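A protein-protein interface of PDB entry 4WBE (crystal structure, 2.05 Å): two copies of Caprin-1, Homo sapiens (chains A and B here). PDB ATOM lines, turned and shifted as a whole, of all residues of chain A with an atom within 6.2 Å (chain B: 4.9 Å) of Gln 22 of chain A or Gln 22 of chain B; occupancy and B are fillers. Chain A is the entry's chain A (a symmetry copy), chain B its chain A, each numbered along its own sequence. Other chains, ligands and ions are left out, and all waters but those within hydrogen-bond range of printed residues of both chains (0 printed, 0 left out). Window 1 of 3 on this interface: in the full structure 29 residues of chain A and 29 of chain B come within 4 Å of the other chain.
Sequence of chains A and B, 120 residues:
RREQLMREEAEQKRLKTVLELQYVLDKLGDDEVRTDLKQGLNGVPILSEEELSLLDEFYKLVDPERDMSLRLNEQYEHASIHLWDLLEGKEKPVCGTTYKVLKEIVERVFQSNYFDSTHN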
ATOM      1  N   THR A  17       8.412 -36.558  20.738  1.00  0.00           N
ATOM      2  CA  THR A  17       9.184 -35.345  20.958  1.00  0.00           C
ATOM      3  C   THR A  17       8.722 -34.224  20.042  1.00  0.00           C
ATOM      4  O   THR A  17       8.618 -33.071  20.474  1.00  0.00           O
ATOM      5  CB  THR A  17      10.694 -35.608  20.779  1.00  0.00           C
ATOM      6  OG1 THR A  17      11.093 -36.657  21.666  1.00  0.00           O
ATOM      7  CG2 THR A  17      11.507 -34.360  21.086  1.00  0.00           C
ATOM      8  N   VAL A  18       8.428 -34.560  18.784  1.00  0.00           N
ATOM      9  CA  VAL A  18       7.895 -33.573  17.854  1.00  0.00           C
ATOM     10  C   VAL A  18       6.579 -32.986  18.370  1.00  0.00           C
ATOM     11  O   VAL A  18       6.379 -31.777  18.337  1.00  0.00           O
ATOM     12  CB  VAL A  18       7.647 -34.170  16.441  1.00  0.00           C
ATOM     13  CG1 VAL A  18       6.916 -33.162  15.574  1.00  0.00           C
ATOM     14  CG2 VAL A  18       8.956 -34.565  15.771  1.00  0.00           C
ATOM     15  N   LEU A  19       5.680 -33.851  18.831  1.00  0.00           N
ATOM     16  CA  LEU A  19       4.384 -33.410  19.355  1.00  0.00           C
ATOM     17  C   LEU A  19       4.541 -32.487  20.569  1.00  0.00           C
ATOM     18  O   LEU A  19       3.872 -31.460  20.674  1.00  0.00           O
ATOM     19  CB  LEU A  19       3.540 -34.630  19.744  1.00  0.00           C
ATOM     20  CG  LEU A  19       2.486 -35.224  18.794  1.00  0.00           C
ATOM     21  CD1 LEU A  19       2.439 -34.588  17.404  1.00  0.00           C
ATOM     22  CD2 LEU A  19       2.597 -36.748  18.718  1.00  0.00           C
ATOM     23  N   GLU A  20       5.418 -32.875  21.488  1.00  0.00           N
ATOM     24  CA  GLU A  20       5.764 -32.049  22.647  1.00  0.00           C
ATOM     25  C   GLU A  20       6.283 -30.682  22.218  1.00  0.00           C
ATOM     26  O   GLU A  20       5.859 -29.646  22.738  1.00  0.00           O
ATOM     27  CB  GLU A  20       6.824 -32.765  23.490  1.00  0.00           C
ATOM     28  CG  GLU A  20       6.331 -34.023  24.184  1.00  0.00           C
ATOM     29  CD  GLU A  20       7.468 -34.957  24.569  1.00  0.00           C
ATOM     30  OE1 GLU A  20       8.646 -34.619  24.324  1.00  0.00           O
ATOM     31  OE2 GLU A  20       7.189 -36.019  25.152  1.00  0.00           O
ATOM     32  N   LEU A  21       7.213 -30.694  21.271  1.00  0.00           N
ATOM     33  CA  LEU A  21       7.789 -29.462  20.753  1.00  0.00           C
ATOM     34  C   LEU A  21       6.733 -28.545  20.135  1.00  0.00           C
ATOM     35  O   LEU A  21       6.740 -27.335  20.364  1.00  0.00           O
ATOM     36  CB  LEU A  21       8.860 -29.788  19.713  1.00  0.00           C
ATOM     37  CG  LEU A  21       9.424 -28.553  19.008  1.00  0.00           C
ATOM     38  CD1 LEU A  21      10.146 -27.660  20.006  1.00  0.00           C
ATOM     39  CD2 LEU A  21      10.364 -28.985  17.893  1.00  0.00           C
ATOM     40  N   GLN A  22       5.830 -29.124  19.350  1.00  0.00           N
ATOM     41  CA  GLN A  22       4.766 -28.353  18.720  1.00  0.00           C
ATOM     42  C   GLN A  22       3.871 -27.719  19.772  1.00  0.00           C
ATOM     43  O   GLN A  22       3.462 -26.563  19.644  1.00  0.00           O
ATOM     44  CB  GLN A  22       3.943 -29.249  17.790  1.00  0.00           C
ATOM     45  CG  GLN A  22       4.702 -29.663  16.534  1.00  0.00           C
ATOM     46  CD  GLN A  22       3.932 -30.641  15.685  1.00  0.00           C
ATOM     47  OE1 GLN A  22       3.227 -31.507  16.202  1.00  0.00           O
ATOM     48  NE2 GLN A  22       4.025 -30.483  14.369  1.00  0.00           N
ATOM     49  N   TYR A  23       3.553 -28.489  20.804  1.00  0.00           N
ATOM     50  CA  TYR A  23       2.774 -27.964  21.912  1.00  0.00           C
ATOM     51  C   TYR A  23       3.469 -26.761  22.548  1.00  0.00           C
ATOM     52  O   TYR A  23       2.859 -25.702  22.738  1.00  0.00           O
ATOM     53  CB  TYR A  23       2.508 -29.053  22.958  1.00  0.00           C
ATOM     54  CG  TYR A  23       1.769 -28.524  24.162  1.00  0.00           C
ATOM     55  CD1 TYR A  23       0.389 -28.385  24.144  1.00  0.00           C
ATOM     56  CD2 TYR A  23       2.449 -28.164  25.317  1.00  0.00           C
ATOM     57  CE1 TYR A  23      -0.295 -27.890  25.242  1.00  0.00           C
ATOM     58  CE2 TYR A  23       1.779 -27.675  26.416  1.00  0.00           C
ATOM     59  CZ  TYR A  23       0.409 -27.540  26.374  1.00  0.00           C
ATOM     60  OH  TYR A  23      -0.256 -27.051  27.475  1.00  0.00           O
ATOM     61  N   VAL A  24       4.743 -26.937  22.892  1.00  0.00           N
ATOM     62  CA  VAL A  24       5.527 -25.865  23.503  1.00  0.00           C
ATOM     63  C   VAL A  24       5.629 -24.636  22.597  1.00  0.00           C
ATOM     64  O   VAL A  24       5.402 -23.515  23.048  1.00  0.00           O
ATOM     65  CB  VAL A  24       6.936 -26.355  23.917  1.00  0.00           C
ATOM     66  CG1 VAL A  24       7.815 -25.187  24.330  1.00  0.00           C
ATOM     67  CG2 VAL A  24       6.824 -27.383  25.041  1.00  0.00           C
ATOM     68  N   LEU A  25       5.977 -24.844  21.328  1.00  0.00           N
ATOM     69  CA  LEU A  25       6.109 -23.728  20.390  1.00  0.00           C
ATOM     70  C   LEU A  25       4.805 -22.943  20.264  1.00  0.00           C
ATOM     71  O   LEU A  25       4.820 -21.719  20.155  1.00  0.00           O
ATOM     72  CB  LEU A  25       6.558 -24.219  19.005  1.00  0.00           C
ATOM     73  CG  LEU A  25       7.987 -24.752  18.898  1.00  0.00           C
ATOM     74  CD1 LEU A  25       8.282 -25.286  17.495  1.00  0.00           C
ATOM     75  CD2 LEU A  25       8.993 -23.688  19.289  1.00  0.00           C
ATOM     76  N   ASP A  26       3.681 -23.653  20.289  1.00  0.00           N
ATOM     77  CA  ASP A  26       2.375 -23.009  20.250  1.00  0.00           C
ATOM     78  C   ASP A  26       2.140 -22.163  21.503  1.00  0.00           C
ATOM     79  O   ASP A  26       1.612 -21.052  21.425  1.00  0.00           O
ATOM     80  CB  ASP A  26       1.267 -24.053  20.101  1.00  0.00           C
ATOM     81  CG  ASP A  26      -0.114 -23.432  20.019  1.00  0.00           C
ATOM     82  OD1 ASP A  26      -0.862 -23.491  21.018  1.00  0.00           O
ATOM     83  OD2 ASP A  26      -0.444 -22.866  18.954  1.00  0.00           O
ATOM     84  N   LYS A  27       2.523 -22.694  22.660  1.00  0.00           N
ATOM     85  CA  LYS A  27       2.340 -21.962  23.911  1.00  0.00           C
ATOM     86  C   LYS A  27       3.241 -20.740  24.032  1.00  0.00           C
ATOM     87  O   LYS A  27       2.920 -19.796  24.753  1.00  0.00           O
ATOM     88  CB  LYS A  27       2.522 -22.892  25.108  1.00  0.00           C
ATOM     89  CG  LYS A  27       1.445 -23.959  25.206  1.00  0.00           C
ATOM     90  CD  LYS A  27       0.076 -23.290  25.288  1.00  0.00           C
ATOM     91  CE  LYS A  27      -0.979 -24.211  25.889  1.00  0.00           C
ATOM     92  NZ  LYS A  27      -2.142 -23.435  26.412  1.00  0.00           N
ATOM     93  N   TYR A  59      10.153 -21.481  14.949  1.00  0.00           N
ATOM     94  CA  TYR A  59       8.719 -21.724  14.842  1.00  0.00           C
ATOM     95  C   TYR A  59       8.212 -21.470  13.426  1.00  0.00           C
ATOM     96  O   TYR A  59       7.435 -22.256  12.890  1.00  0.00           O
ATOM     97  CB  TYR A  59       7.969 -20.789  15.795  1.00  0.00           C
ATOM     98  CG  TYR A  59       6.461 -20.911  15.710  1.00  0.00           C
ATOM     99  CD1 TYR A  59       5.820 -22.121  15.936  1.00  0.00           C
ATOM    100  CD2 TYR A  59       5.686 -19.817  15.329  1.00  0.00           C
ATOM    101  CE1 TYR A  59       4.435 -22.228  15.842  1.00  0.00           C
ATOM    102  CE2 TYR A  59       4.308 -19.911  15.220  1.00  0.00           C
ATOM    103  CZ  TYR A  59       3.688 -21.120  15.476  1.00  0.00           C
ATOM    104  OH  TYR A  59       2.318 -21.213  15.368  1.00  0.00           O
ATOM    105  N   VAL A  62       9.237 -24.412  11.008  1.00  0.00           N
ATOM    106  CA  VAL A  62       8.613 -25.720  11.136  1.00  0.00           C
ATOM    107  C   VAL A  62       7.093 -25.664  11.104  1.00  0.00           C
ATOM    108  O   VAL A  62       6.437 -26.695  10.947  1.00  0.00           O
ATOM    109  CB  VAL A  62       9.125 -26.493  12.371  1.00  0.00           C
ATOM    110  CG1 VAL A  62      10.611 -26.736  12.239  1.00  0.00           C
ATOM    111  CG2 VAL A  62       8.820 -25.730  13.654  1.00  0.00           C
ATOM    112  N   LEU A  83      12.907 -30.045  11.530  1.00  0.00           N
ATOM    113  CA  LEU A  83      12.523 -30.813  12.705  1.00  0.00           C
ATOM    114  C   LEU A  83      13.497 -31.954  12.965  1.00  0.00           C
ATOM    115  O   LEU A  83      13.922 -32.174  14.101  1.00  0.00           O
ATOM    116  CB  LEU A  83      11.114 -31.380  12.524  1.00  0.00           C
ATOM    117  CG  LEU A  83       9.975 -30.388  12.747  1.00  0.00           C
ATOM    118  CD1 LEU A  83       8.644 -31.031  12.408  1.00  0.00           C
ATOM    119  CD2 LEU A  83       9.987 -29.890  14.182  1.00  0.00           C
ATOM    120  N   VAL B  18       3.444 -36.604   8.503  1.00  0.00           N
ATOM    121  CA  VAL B  18       2.780 -36.214   9.740  1.00  0.00           C
ATOM    122  C   VAL B  18       2.319 -34.755   9.678  1.00  0.00           C
ATOM    123  O   VAL B  18       1.194 -34.439  10.050  1.00  0.00           O
ATOM    124  CB  VAL B  18       3.698 -36.387  10.982  1.00  0.00           C
ATOM    125  CG1 VAL B  18       3.032 -35.788  12.206  1.00  0.00           C
ATOM    126  CG2 VAL B  18       4.008 -37.856  11.237  1.00  0.00           C
ATOM    127  N   LEU B  19       3.200 -33.869   9.222  1.00  0.00           N
ATOM    128  CA  LEU B  19       2.875 -32.445   9.112  1.00  0.00           C
ATOM    129  C   LEU B  19       1.701 -32.196   8.158  1.00  0.00           C
ATOM    130  O   LEU B  19       0.799 -31.415   8.456  1.00  0.00           O
ATOM    131  CB  LEU B  19       4.105 -31.668   8.625  1.00  0.00           C
ATOM    132  CG  LEU B  19       5.052 -30.952   9.602  1.00  0.00           C
ATOM    133  CD1 LEU B  19       4.745 -31.180  11.082  1.00  0.00           C
ATOM    134  CD2 LEU B  19       6.518 -31.243   9.274  1.00  0.00           C
ATOM    135  N   GLU B  20       1.735 -32.857   7.007  1.00  0.00           N
ATOM    136  CA  GLU B  20       0.635 -32.815   6.040  1.00  0.00           C
ATOM    137  C   GLU B  20      -0.675 -33.272   6.672  1.00  0.00           C
ATOM    138  O   GLU B  20      -1.715 -32.623   6.526  1.00  0.00           O
ATOM    139  CB  GLU B  20       0.971 -33.705   4.840  1.00  0.00           C
ATOM    140  CG  GLU B  20       2.115 -33.196   3.980  1.00  0.00           C
ATOM    141  CD  GLU B  20       2.746 -34.298   3.142  1.00  0.00           C
ATOM    142  OE1 GLU B  20       2.280 -35.456   3.205  1.00  0.00           O
ATOM    143  OE2 GLU B  20       3.689 -34.001   2.389  1.00  0.00           O
ATOM    144  N   LEU B  21      -0.612 -34.402   7.365  1.00  0.00           N
ATOM    145  CA  LEU B  21      -1.782 -34.951   8.035  1.00  0.00           C
ATOM    146  C   LEU B  21      -2.361 -33.986   9.071  1.00  0.00           C
ATOM    147  O   LEU B  21      -3.576 -33.805   9.151  1.00  0.00           O
ATOM    148  CB  LEU B  21      -1.421 -36.274   8.708  1.00  0.00           C
ATOM    149  CG  LEU B  21      -2.551 -36.856   9.558  1.00  0.00           C
ATOM    150  CD1 LEU B  21      -3.743 -37.209   8.680  1.00  0.00           C
ATOM    151  CD2 LEU B  21      -2.050 -38.083  10.304  1.00  0.00           C
ATOM    152  N   GLN B  22      -1.488 -33.373   9.864  1.00  0.00           N
ATOM    153  CA  GLN B  22      -1.921 -32.419  10.877  1.00  0.00           C
ATOM    154  C   GLN B  22      -2.611 -31.229  10.230  1.00  0.00           C
ATOM    155  O   GLN B  22      -3.630 -30.741  10.724  1.00  0.00           O
ATOM    156  CB  GLN B  22      -0.725 -31.954  11.711  1.00  0.00           C
ATOM    157  CG  GLN B  22      -0.181 -33.039  12.633  1.00  0.00           C
ATOM    158  CD  GLN B  22       1.068 -32.612  13.360  1.00  0.00           C
ATOM    159  OE1 GLN B  22       1.906 -31.900  12.809  1.00  0.00           O
ATOM    160  NE2 GLN B  22       1.182 -33.010  14.623  1.00  0.00           N
ATOM    161  N   TYR B  23      -2.039 -30.753   9.133  1.00  0.00           N
ATOM    162  CA  TYR B  23      -2.654 -29.672   8.382  1.00  0.00           C
ATOM    163  C   TYR B  23      -4.062 -30.055   7.928  1.00  0.00           C
ATOM    164  O   TYR B  23      -5.023 -29.305   8.140  1.00  0.00           O
ATOM    165  CB  TYR B  23      -1.786 -29.277   7.182  1.00  0.00           C
ATOM    166  CG  TYR B  23      -2.431 -28.211   6.332  1.00  0.00           C
ATOM    167  CD1 TYR B  23      -2.336 -26.872   6.679  1.00  0.00           C
ATOM    168  CD2 TYR B  23      -3.137 -28.543   5.184  1.00  0.00           C
ATOM    169  CE1 TYR B  23      -2.937 -25.888   5.909  1.00  0.00           C
ATOM    170  CE2 TYR B  23      -3.733 -27.573   4.408  1.00  0.00           C
ATOM    171  CZ  TYR B  23      -3.630 -26.250   4.774  1.00  0.00           C
ATOM    172  OH  TYR B  23      -4.229 -25.285   3.996  1.00  0.00           O
ATOM    173  N   VAL B  24      -4.174 -31.216   7.287  1.00  0.00           N
ATOM    174  CA  VAL B  24      -5.465 -31.704   6.805  1.00  0.00           C
ATOM    175  C   VAL B  24      -6.472 -31.892   7.943  1.00  0.00           C
ATOM    176  O   VAL B  24      -7.611 -31.440   7.842  1.00  0.00           O
ATOM    177  CB  VAL B  24      -5.312 -33.012   5.992  1.00  0.00           C
ATOM    178  CG1 VAL B  24      -6.670 -33.630   5.701  1.00  0.00           C
ATOM    179  CG2 VAL B  24      -4.545 -32.739   4.700  1.00  0.00           C
ATOM    180  N   LEU B  25      -6.057 -32.562   9.017  1.00  0.00           N
ATOM    181  CA  LEU B  25      -6.953 -32.799  10.151  1.00  0.00           C
ATOM    182  C   LEU B  25      -7.469 -31.489  10.741  1.00  0.00           C
ATOM    183  O   LEU B  25      -8.626 -31.398  11.143  1.00  0.00           O
ATOM    184  CB  LEU B  25      -6.256 -33.626  11.243  1.00  0.00           C
ATOM    185  CG  LEU B  25      -5.954 -35.087  10.906  1.00  0.00           C
ATOM    186  CD1 LEU B  25      -5.188 -35.774  12.038  1.00  0.00           C
ATOM    187  CD2 LEU B  25      -7.226 -35.843  10.583  1.00  0.00           C
ATOM    188  N   ASP B  26      -6.607 -30.477  10.784  1.00  0.00           N
ATOM    189  CA  ASP B  26      -7.005 -29.159  11.259  1.00  0.00           C
ATOM    190  C   ASP B  26      -8.049 -28.533  10.333  1.00  0.00           C
ATOM    191  O   ASP B  26      -9.016 -27.922  10.794  1.00  0.00           O
ATOM    192  CB  ASP B  26      -5.787 -28.242  11.380  1.00  0.00           C
ATOM    193  CG  ASP B  26      -6.142 -26.865  11.906  1.00  0.00           C
ATOM    194  OD1 ASP B  26      -6.177 -25.905  11.106  1.00  0.00           O
ATOM    195  OD2 ASP B  26      -6.405 -26.749  13.122  1.00  0.00           O
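Hydrophobic or aromatic side chains of chain A within 4 Å of the printed part of chain B: Leu 19 and Leu 83.
Of the 9 printed residues of chain B, 2 touch a printed residue of chain A.
Printed residues of chain B that touch a printed residue of chain A: Leu 19 and Gln 22.
Among the printed residues, 4 pairs touch across the chains.
Leu 19 of chain A touches Gln 22 of chain B, and with the chains exchanged Gln 22 of chain A touches Leu 19 of chain B.
Gln 22 of chain B touches its own counterpart, Gln 22 of chain A.
9 positions are printed for both chains.
Of the 4 pairs that touch across the chains among the printed residues, 3 have their exchanged pair printed and touching as well.
NE2 of Gln 22 of chain B sits at hydrogen-bond distance from OE1 of Gln 22 of chain A.
Among the printed residues, pairs that only touch across the chains: Leu 19 of chain A with Gln 22 of chain B (3.4 Å), Gln 22 of chain A with Leu 19 of chain B (3.4 Å) and Leu 83 of chain A with Leu 19 of chain B (3.8 Å).
Asp 26 of chain A touches none of the printed residues of chain B.
Of the printed residues of chain B, Leu 83 of chain A touches Leu 19 (3.8 Å).
Of the printed residues of chain A, Leu 19 of chain B touches Gln 22 (3.4 Å) and Leu 83 (3.8 Å).
Gln 22 of chain B touches just these residues of chain A: Leu 19 (3.4 Å) and Gln 22 (3.0 Å).
The nearest printed residue of chain B that does not touch Gln 22 of chain A is Val 18 of chain B (5.8 Å).
The nearest residue of chain A that does not touch Gln 22 of chain B is Val 18 of chain A (5.8 Å).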
